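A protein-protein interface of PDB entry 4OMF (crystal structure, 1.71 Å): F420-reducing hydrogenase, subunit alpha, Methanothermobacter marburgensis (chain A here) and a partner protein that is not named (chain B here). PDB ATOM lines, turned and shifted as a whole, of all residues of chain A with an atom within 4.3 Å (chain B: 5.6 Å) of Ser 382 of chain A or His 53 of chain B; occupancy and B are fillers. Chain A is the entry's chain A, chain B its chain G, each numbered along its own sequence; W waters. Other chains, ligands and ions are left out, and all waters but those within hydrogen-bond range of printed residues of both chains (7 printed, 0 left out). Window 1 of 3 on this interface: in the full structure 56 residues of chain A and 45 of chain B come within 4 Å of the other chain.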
ATOM      1  N   GLU A  14      16.011 -11.006  -5.969  1.00  0.00           N
ATOM      2  CA  GLU A  14      17.111 -10.041  -5.867  1.00  0.00           C
ATOM      3  C   GLU A  14      17.277  -9.581  -4.428  1.00  0.00           C
ATOM      4  O   GLU A  14      16.297  -9.238  -3.777  1.00  0.00           O
ATOM      5  CB  GLU A  14      16.877  -8.833  -6.766  1.00  0.00           C
ATOM      6  CG  GLU A  14      18.123  -7.947  -6.978  1.00  0.00           C
ATOM      7  CD  GLU A  14      18.495  -7.100  -5.765  1.00  0.00           C
ATOM      8  OE1 GLU A  14      17.605  -6.802  -4.928  1.00  0.00           O
ATOM      9  OE2 GLU A  14      19.693  -6.748  -5.647  1.00  0.00           O
ATOM     10  N   GLY A  15      18.517  -9.555  -3.954  1.00  0.00           N
ATOM     11  CA  GLY A  15      18.847  -8.941  -2.677  1.00  0.00           C
ATOM     12  C   GLY A  15      18.421  -9.744  -1.464  1.00  0.00           C
ATOM     13  O   GLY A  15      17.814 -10.815  -1.603  1.00  0.00           O
ATOM     14  N   HIS A  16      18.739  -9.224  -0.276  1.00  0.00           N
ATOM     15  CA  HIS A  16      18.610  -9.999   0.954  1.00  0.00           C
ATOM     16  C   HIS A  16      17.505  -9.538   1.895  1.00  0.00           C
ATOM     17  O   HIS A  16      17.485  -8.398   2.345  1.00  0.00           O
ATOM     18  CB  HIS A  16      19.961  -9.994   1.680  1.00  0.00           C
ATOM     19  CG  HIS A  16      21.052 -10.600   0.854  1.00  0.00           C
ATOM     20  ND1 HIS A  16      20.883 -11.789   0.170  1.00  0.00           N
ATOM     21  CD2 HIS A  16      22.302 -10.169   0.563  1.00  0.00           C
ATOM     22  CE1 HIS A  16      21.990 -12.064  -0.505  1.00  0.00           C
ATOM     23  NE2 HIS A  16      22.875 -11.109  -0.262  1.00  0.00           N
ATOM     24  N   ARG A  41      22.106   1.744   1.401  1.00  0.00           N
ATOM     25  CA  ARG A  41      23.024   2.588   0.632  1.00  0.00           C
ATOM     26  C   ARG A  41      22.580   4.064   0.691  1.00  0.00           C
ATOM     27  O   ARG A  41      23.406   4.967   0.675  1.00  0.00           O
ATOM     28  CB  ARG A  41      23.123   2.050  -0.811  1.00  0.00           C
ATOM     29  CG  ARG A  41      23.909   0.714  -0.834  1.00  0.00           C
ATOM     30  CD  ARG A  41      23.791  -0.098  -2.095  1.00  0.00           C
ATOM     31  NE  ARG A  41      22.382  -0.275  -2.404  1.00  0.00           N
ATOM     32  CZ  ARG A  41      21.858  -0.281  -3.629  1.00  0.00           C
ATOM     33  NH1 ARG A  41      22.619  -0.176  -4.722  1.00  0.00           N
ATOM     34  NH2 ARG A  41      20.549  -0.397  -3.754  1.00  0.00           N
ATOM     35  N   ILE A  62      19.986   2.031  -7.783  1.00  0.00           N
ATOM     36  CA  ILE A  62      19.236   1.305  -6.752  1.00  0.00           C
ATOM     37  C   ILE A  62      19.222  -0.191  -7.093  1.00  0.00           C
ATOM     38  O   ILE A  62      19.361  -1.061  -6.207  1.00  0.00           O
ATOM     39  CB  ILE A  62      17.797   1.818  -6.653  1.00  0.00           C
ATOM     40  CG1 ILE A  62      17.744   3.189  -5.955  1.00  0.00           C
ATOM     41  CG2 ILE A  62      16.886   0.763  -5.974  1.00  0.00           C
ATOM     42  CD1 ILE A  62      16.359   3.907  -6.068  1.00  0.00           C
ATOM     43  N   CYS A 380      12.458  -7.564  -4.876  1.00  0.00           N
ATOM     44  CA  CYS A 380      13.739  -6.960  -5.166  1.00  0.00           C
ATOM     45  C   CYS A 380      14.150  -6.132  -3.956  1.00  0.00           C
ATOM     46  O   CYS A 380      13.524  -5.107  -3.670  1.00  0.00           O
ATOM     47  CB  CYS A 380      13.644  -6.112  -6.418  1.00  0.00           C
ATOM     48  SG  CYS A 380      15.298  -5.640  -6.843  1.00  0.00           S
ATOM     49  N   LEU A 381      15.176  -6.598  -3.231  1.00  0.00           N
ATOM     50  CA  LEU A 381      15.447  -6.029  -1.909  1.00  0.00           C
ATOM     51  C   LEU A 381      16.399  -4.839  -2.019  1.00  0.00           C
ATOM     52  O   LEU A 381      16.314  -3.926  -1.206  1.00  0.00           O
ATOM     53  CB  LEU A 381      15.987  -7.095  -0.959  1.00  0.00           C
ATOM     54  CG  LEU A 381      14.886  -7.740  -0.107  1.00  0.00           C
ATOM     55  CD1 LEU A 381      14.554  -6.770   1.021  1.00  0.00           C
ATOM     56  CD2 LEU A 381      13.579  -7.996  -0.900  1.00  0.00           C
ATOM     57  N   SER A 382      17.251  -4.801  -3.042  1.00  0.00           N
ATOM     58  CA  SER A 382      18.020  -3.571  -3.269  1.00  0.00           C
ATOM     59  C   SER A 382      17.044  -2.453  -3.640  1.00  0.00           C
ATOM     60  O   SER A 382      17.145  -1.342  -3.139  1.00  0.00           O
ATOM     61  CB  SER A 382      19.087  -3.754  -4.345  1.00  0.00           C
ATOM     62  OG  SER A 382      20.025  -4.730  -3.957  1.00  0.00           O
ATOM     63  N   CYS A 383      16.066  -2.776  -4.479  1.00  0.00           N
ATOM     64  CA  CYS A 383      14.930  -1.867  -4.720  1.00  0.00           C
ATOM     65  C   CYS A 383      14.175  -1.435  -3.479  1.00  0.00           C
ATOM     66  O   CYS A 383      13.927  -0.242  -3.276  1.00  0.00           O
ATOM     67  CB  CYS A 383      13.943  -2.524  -5.650  1.00  0.00           C
ATOM     68  SG  CYS A 383      14.233  -2.046  -7.302  1.00  0.00           S
ATOM     69  N   ALA A 384      13.751  -2.405  -2.675  1.00  0.00           N
ATOM     70  CA  ALA A 384      12.971  -2.106  -1.476  1.00  0.00           C
ATOM     71  C   ALA A 384      13.672  -1.133  -0.521  1.00  0.00           C
ATOM     72  O   ALA A 384      13.012  -0.342   0.168  1.00  0.00           O
ATOM     73  CB  ALA A 384      12.627  -3.409  -0.731  1.00  0.00           C
ATOM     74  N   THR A 385      14.996  -1.201  -0.498  1.00  0.00           N
ATOM     75  CA  THR A 385      15.769  -0.563   0.557  1.00  0.00           C
ATOM     76  C   THR A 385      16.401   0.748   0.097  1.00  0.00           C
ATOM     77  O   THR A 385      16.361   1.743   0.813  1.00  0.00           O
ATOM     78  CB  THR A 385      16.846  -1.552   1.050  1.00  0.00           C
ATOM     79  OG1 THR A 385      16.202  -2.811   1.340  1.00  0.00           O
ATOM     80  CG2 THR A 385      17.575  -1.007   2.272  1.00  0.00           C
ATOM     81  N   HIS A 386      16.958   0.734  -1.120  1.00  0.00           N
ATOM     82  CA  HIS A 386      17.581   1.892  -1.767  1.00  0.00           C
ATOM     83  C   HIS A 386      18.402   2.756  -0.798  1.00  0.00           C
ATOM     84  O   HIS A 386      18.305   3.983  -0.734  1.00  0.00           O
ATOM     85  CB  HIS A 386      16.519   2.737  -2.568  1.00  0.00           C
ATOM     86  CG  HIS A 386      15.206   2.996  -1.863  1.00  0.00           C
ATOM     87  ND1 HIS A 386      14.135   2.118  -1.890  1.00  0.00           N
ATOM     88  CD2 HIS A 386      14.775   4.084  -1.176  1.00  0.00           C
ATOM     89  CE1 HIS A 386      13.120   2.641  -1.219  1.00  0.00           C
ATOM     90  NE2 HIS A 386      13.475   3.844  -0.793  1.00  0.00           N
ATOM     91  N   TYR B  51      28.598 -16.728  -6.102  1.00  0.00           N
ATOM     92  CA  TYR B  51      28.214 -15.367  -6.425  1.00  0.00           C
ATOM     93  C   TYR B  51      27.659 -14.746  -5.164  1.00  0.00           C
ATOM     94  O   TYR B  51      26.552 -15.100  -4.740  1.00  0.00           O
ATOM     95  CB  TYR B  51      27.172 -15.311  -7.544  1.00  0.00           C
ATOM     96  CG  TYR B  51      26.454 -13.974  -7.589  1.00  0.00           C
ATOM     97  CD1 TYR B  51      25.090 -13.886  -7.316  1.00  0.00           C
ATOM     98  CD2 TYR B  51      27.149 -12.793  -7.861  1.00  0.00           C
ATOM     99  CE1 TYR B  51      24.429 -12.666  -7.327  1.00  0.00           C
ATOM    100  CE2 TYR B  51      26.490 -11.557  -7.876  1.00  0.00           C
ATOM    101  CZ  TYR B  51      25.128 -11.512  -7.604  1.00  0.00           C
ATOM    102  OH  TYR B  51      24.459 -10.306  -7.614  1.00  0.00           O
ATOM    103  N   ILE B  52      28.434 -13.857  -4.544  1.00  0.00           N
ATOM    104  CA  ILE B  52      28.037 -13.250  -3.269  1.00  0.00           C
ATOM    105  C   ILE B  52      27.692 -11.782  -3.460  1.00  0.00           C
ATOM    106  O   ILE B  52      28.524 -10.993  -3.877  1.00  0.00           O
ATOM    107  CB  ILE B  52      29.142 -13.355  -2.197  1.00  0.00           C
ATOM    108  CG1 ILE B  52      29.424 -14.811  -1.838  1.00  0.00           C
ATOM    109  CG2 ILE B  52      28.720 -12.602  -0.940  1.00  0.00           C
ATOM    110  CD1 ILE B  52      30.470 -15.488  -2.704  1.00  0.00           C
ATOM    111  N   HIS B  53      26.456 -11.433  -3.138  1.00  0.00           N
ATOM    112  CA  HIS B  53      25.951 -10.082  -3.323  1.00  0.00           C
ATOM    113  C   HIS B  53      26.023  -9.363  -1.960  1.00  0.00           C
ATOM    114  O   HIS B  53      25.369  -9.800  -0.997  1.00  0.00           O
ATOM    115  CB  HIS B  53      24.520 -10.164  -3.903  1.00  0.00           C
ATOM    116  CG  HIS B  53      23.722  -8.912  -3.769  1.00  0.00           C
ATOM    117  ND1 HIS B  53      23.704  -7.934  -4.739  1.00  0.00           N
ATOM    118  CD2 HIS B  53      22.890  -8.489  -2.789  1.00  0.00           C
ATOM    119  CE1 HIS B  53      22.916  -6.949  -4.351  1.00  0.00           C
ATOM    120  NE2 HIS B  53      22.398  -7.267  -3.177  1.00  0.00           N
ATOM    121  N   LEU B  54      26.858  -8.314  -1.865  1.00  0.00           N
ATOM    122  CA  LEU B  54      26.938  -7.473  -0.662  1.00  0.00           C
ATOM    123  C   LEU B  54      26.106  -6.231  -0.941  1.00  0.00           C
ATOM    124  O   LEU B  54      24.936  -6.367  -1.297  1.00  0.00           O
ATOM    125  CB  LEU B  54      28.397  -7.141  -0.299  1.00  0.00           C
ATOM    126  CG  LEU B  54      29.315  -8.351  -0.022  1.00  0.00           C
ATOM    127  CD1 LEU B  54      30.805  -7.958   0.151  1.00  0.00           C
ATOM    128  CD2 LEU B  54      28.852  -9.138   1.222  1.00  0.00           C
ATOM    129  N   SER B  55      26.664  -5.037  -0.813  1.00  0.00           N
ATOM    130  CA  SER B  55      25.848  -3.848  -1.121  1.00  0.00           C
ATOM    131  C   SER B  55      26.011  -3.487  -2.593  1.00  0.00           C
ATOM    132  O   SER B  55      26.610  -2.453  -2.944  1.00  0.00           O
ATOM    133  CB  SER B  55      26.204  -2.675  -0.200  1.00  0.00           C
ATOM    134  OG  SER B  55      25.816  -2.967   1.145  1.00  0.00           O
ATOM    135  N   GLY B  56      25.473  -4.366  -3.442  1.00  0.00           N
ATOM    136  CA  GLY B  56      25.503  -4.209  -4.881  1.00  0.00           C
ATOM    137  C   GLY B  56      24.097  -3.940  -5.350  1.00  0.00           C
ATOM    138  O   GLY B  56      23.235  -3.654  -4.534  1.00  0.00           O
ATOM    139  N   CYS B  57      23.872  -3.992  -6.664  1.00  0.00           N
ATOM    140  CA  CYS B  57      22.539  -3.753  -7.212  1.00  0.00           C
ATOM    141  C   CYS B  57      22.096  -4.940  -8.080  1.00  0.00           C
ATOM    142  O   CYS B  57      21.008  -4.928  -8.667  1.00  0.00           O
ATOM    143  CB  CYS B  57      22.504  -2.459  -8.029  1.00  0.00           C
ATOM    144  SG  CYS B  57      23.205  -2.739  -9.711  1.00  0.00           S
ATOM    145  N   THR B  58      22.956  -5.965  -8.112  1.00  0.00           N
ATOM    146  CA  THR B  58      22.784  -7.204  -8.864  1.00  0.00           C
ATOM    147  C   THR B  58      22.935  -7.001 -10.380  1.00  0.00           C
ATOM    148  O   THR B  58      22.800  -7.940 -11.172  1.00  0.00           O
ATOM    149  CB  THR B  58      21.435  -7.886  -8.478  1.00  0.00           C
ATOM    150  OG1 THR B  58      21.427  -8.062  -7.056  1.00  0.00           O
ATOM    151  CG2 THR B  58      21.276  -9.272  -9.098  1.00  0.00           C
ATOM    152  N   THR B  86      21.087 -15.697  -4.217  1.00  0.00           N
ATOM    153  CA  THR B  86      20.411 -15.163  -5.404  1.00  0.00           C
ATOM    154  C   THR B  86      20.104 -16.293  -6.391  1.00  0.00           C
ATOM    155  O   THR B  86      19.084 -16.262  -7.081  1.00  0.00           O
ATOM    156  CB  THR B  86      21.253 -14.082  -6.130  1.00  0.00           C
ATOM    157  OG1 THR B  86      21.718 -13.075  -5.199  1.00  0.00           O
ATOM    158  CG2 THR B  86      20.412 -13.407  -7.205  1.00  0.00           C
ATOM    159  N   LEU B 100      32.799 -14.570  -6.908  1.00  0.00           N
ATOM    160  CA  LEU B 100      32.476 -13.326  -7.586  1.00  0.00           C
ATOM    161  C   LEU B 100      31.717 -12.476  -6.576  1.00  0.00           C
ATOM    162  O   LEU B 100      30.583 -12.818  -6.220  1.00  0.00           O
ATOM    163  CB  LEU B 100      31.620 -13.585  -8.838  1.00  0.00           C
ATOM    164  CG  LEU B 100      32.252 -14.327 -10.015  1.00  0.00           C
ATOM    165  CD1 LEU B 100      31.152 -14.705 -11.000  1.00  0.00           C
ATOM    166  CD2 LEU B 100      33.285 -13.439 -10.697  1.00  0.00           C
ATOM    167  N   GLU B 102      30.012  -9.154  -5.499  1.00  0.00           N
ATOM    168  CA  GLU B 102      29.413  -7.969  -6.060  1.00  0.00           C
ATOM    169  C   GLU B 102      29.014  -6.978  -4.954  1.00  0.00           C
ATOM    170  O   GLU B 102      28.473  -7.390  -3.923  1.00  0.00           O
ATOM    171  CB  GLU B 102      28.195  -8.369  -6.886  1.00  0.00           C
ATOM    172  CG  GLU B 102      27.416  -7.167  -7.357  1.00  0.00           C
ATOM    173  CD  GLU B 102      26.012  -7.558  -7.661  1.00  0.00           C
ATOM    174  OE1 GLU B 102      25.819  -8.276  -8.667  1.00  0.00           O
ATOM    175  OE2 GLU B 102      25.118  -7.178  -6.869  1.00  0.00           O
HETATM  176  O   HOH W   1      20.854 -10.196  -5.487  1.00  0.00           O
HETATM  177  O   HOH W   2      24.758 -13.179  -1.678  1.00  0.00           O
HETATM  178  O   HOH W   3      25.512  -0.826  -4.964  1.00  0.00           O
HETATM  179  O   HOH W   4      19.646 -12.513  -3.574  1.00  0.00           O
HETATM  180  O   HOH W   5      25.631 -10.637   1.776  1.00  0.00           O
HETATM  181  O   HOH W   6      22.049  -3.807  -1.961  1.00  0.00           O
HETATM  182  O   HOH W   7      20.670  -7.113  -0.649  1.00  0.00           O
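O of Gly 56 of chain B lies within hydrogen-bond range of OG of Ser 382 of chain A (3.4 Å).
NE2 of His 16 of chain A is in hydrogen-bond range of O of His 53 of chain B.
The side-chain carboxylate (OE2) of Glu 14 of chain A is in hydrogen-bond range of the side-chain hydroxyl (OG1) of Thr 58 of chain B (2.6 Å).
Among the printed residues, pairs that only touch across the chains: Glu 14 of chain A with His 53 of chain B, Arg 41 of chain A with Gly 56 of chain B, Ser 382 of chain A with His 53 of chain B, Glu 14 of chain A with Cys 57 of chain B, Arg 41 of chain A with Ser 55 of chain B, Ile 62 of chain A with Cys 57 of chain B and Gly 15 of chain A with His 53 of chain B.
Hydrophobic or aromatic side chains of chain A that line the printed part of chain B: His 16.
Of the 11 printed residues of chain B, 5 touch a printed residue of chain A.
Printed residues of chain B that touch a printed residue of chain A: His 53, Ser 55, Gly 56, Cys 57 and Thr 58.
Hydrophobic or aromatic side chains of chain B that line the printed part of chain A: His 53.
Among the printed residues, 10 pairs touch across the chains.
Among the printed residues, no Asp or Glu carboxylate lies within 4 Å of a Lys or Arg side-chain nitrogen of the other chain.
Of the printed residues of chain B, Gly 15 of chain A touches His 53 (3.96 Å).
Printed residues of chain B within 4 Å of His 16 of chain A: His 53 (2.9 Å).
Leu 381 of chain A touches none of the printed residues of chain B.
Ser 382 of chain A touches just these residues of chain B: His 53 (3.6 Å) and Gly 56 (3.4 Å).
His 53 of chain B touches four residues of chain A.
Of the printed residues of chain A, Ser 55 of chain B touches Arg 41 (3.8 Å).
Of the printed residues of chain A, Gly 56 of chain B touches Arg 41 and Ser 382.
Printed residues of chain A within 4 Å of Cys 57 of chain B: Glu 14 and Ile 62.
The nearest residue of chain B that does not touch Ser 382 of chain A is Cys 57 of chain B (4.2 Å).
The nearest printed residue of chain A that does not touch His 53 of chain B is Leu 381 of chain A (6.6 Å).
The nearest printed residue of chain B that does not touch Gly 15 of chain A is Thr 58 of chain B (4.5 Å).
Water W4 bridges OG1 of Thr 86 of chain B (2.7 Å) and O of Gly 15 of chain A (3.2 Å).
Water W1 lies within hydrogen-bond range of the side-chain hydroxyl of Thr 58 of chain B (2.7 Å), the backbone NH of Gly 15 of chain A (2.9 Å) and the side-chain hydroxyl of Thr 86 of chain B (3.0 Å).
Water W3 bridges O of Ser 55 of chain B (2.8 Å) and NH1 of Arg 41 of chain A (3.0 Å).
Water W6 bridges the backbone carbonyl oxygen (O) of Gly 56 of chain B (2.8 Å) and the side-chain hydroxyl (OG) of Ser 382 of chain A (3.0 Å).
Water W2 lies within hydrogen-bond range of the backbone NH of His 53 of chain B (2.8 Å) and a ring nitrogen (NE2) of His 16 of chain A (3.1 Å).
Water W7 bridges the backbone NH (N) of His 16 of chain A (2.9 Å) and a ring nitrogen (NE2) of His 53 of chain B (3.1 Å).
A ring nitrogen (ND1) of His 53 of chain B sits at hydrogen-bond distance from the side-chain hydroxyl of Thr 58 of chain B.
The backbone NH (N) of Thr 58 of chain B is in hydrogen-bond range of the side-chain carboxylate (OE2) of Glu 102 of chain B, at 2.8 Å.
The backbone NH of Leu 381 of chain A is in hydrogen-bond range of the backbone carbonyl oxygen of Glu 14 of chain A, 2.9 Å away.
The side-chain carboxylate of Glu 102 of chain B lies within hydrogen-bond range of the backbone NH of Cys 57 of chain B.
The side-chain carboxylate of Glu 14 of chain A is in hydrogen-bond range of the side-chain hydroxyl of Ser 382 of chain A, 2.7 Å away.
A ring nitrogen (ND1) of His 53 of chain B lies within hydrogen-bond range of the side-chain carboxylate (OE2) of Glu 102 of chain B.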
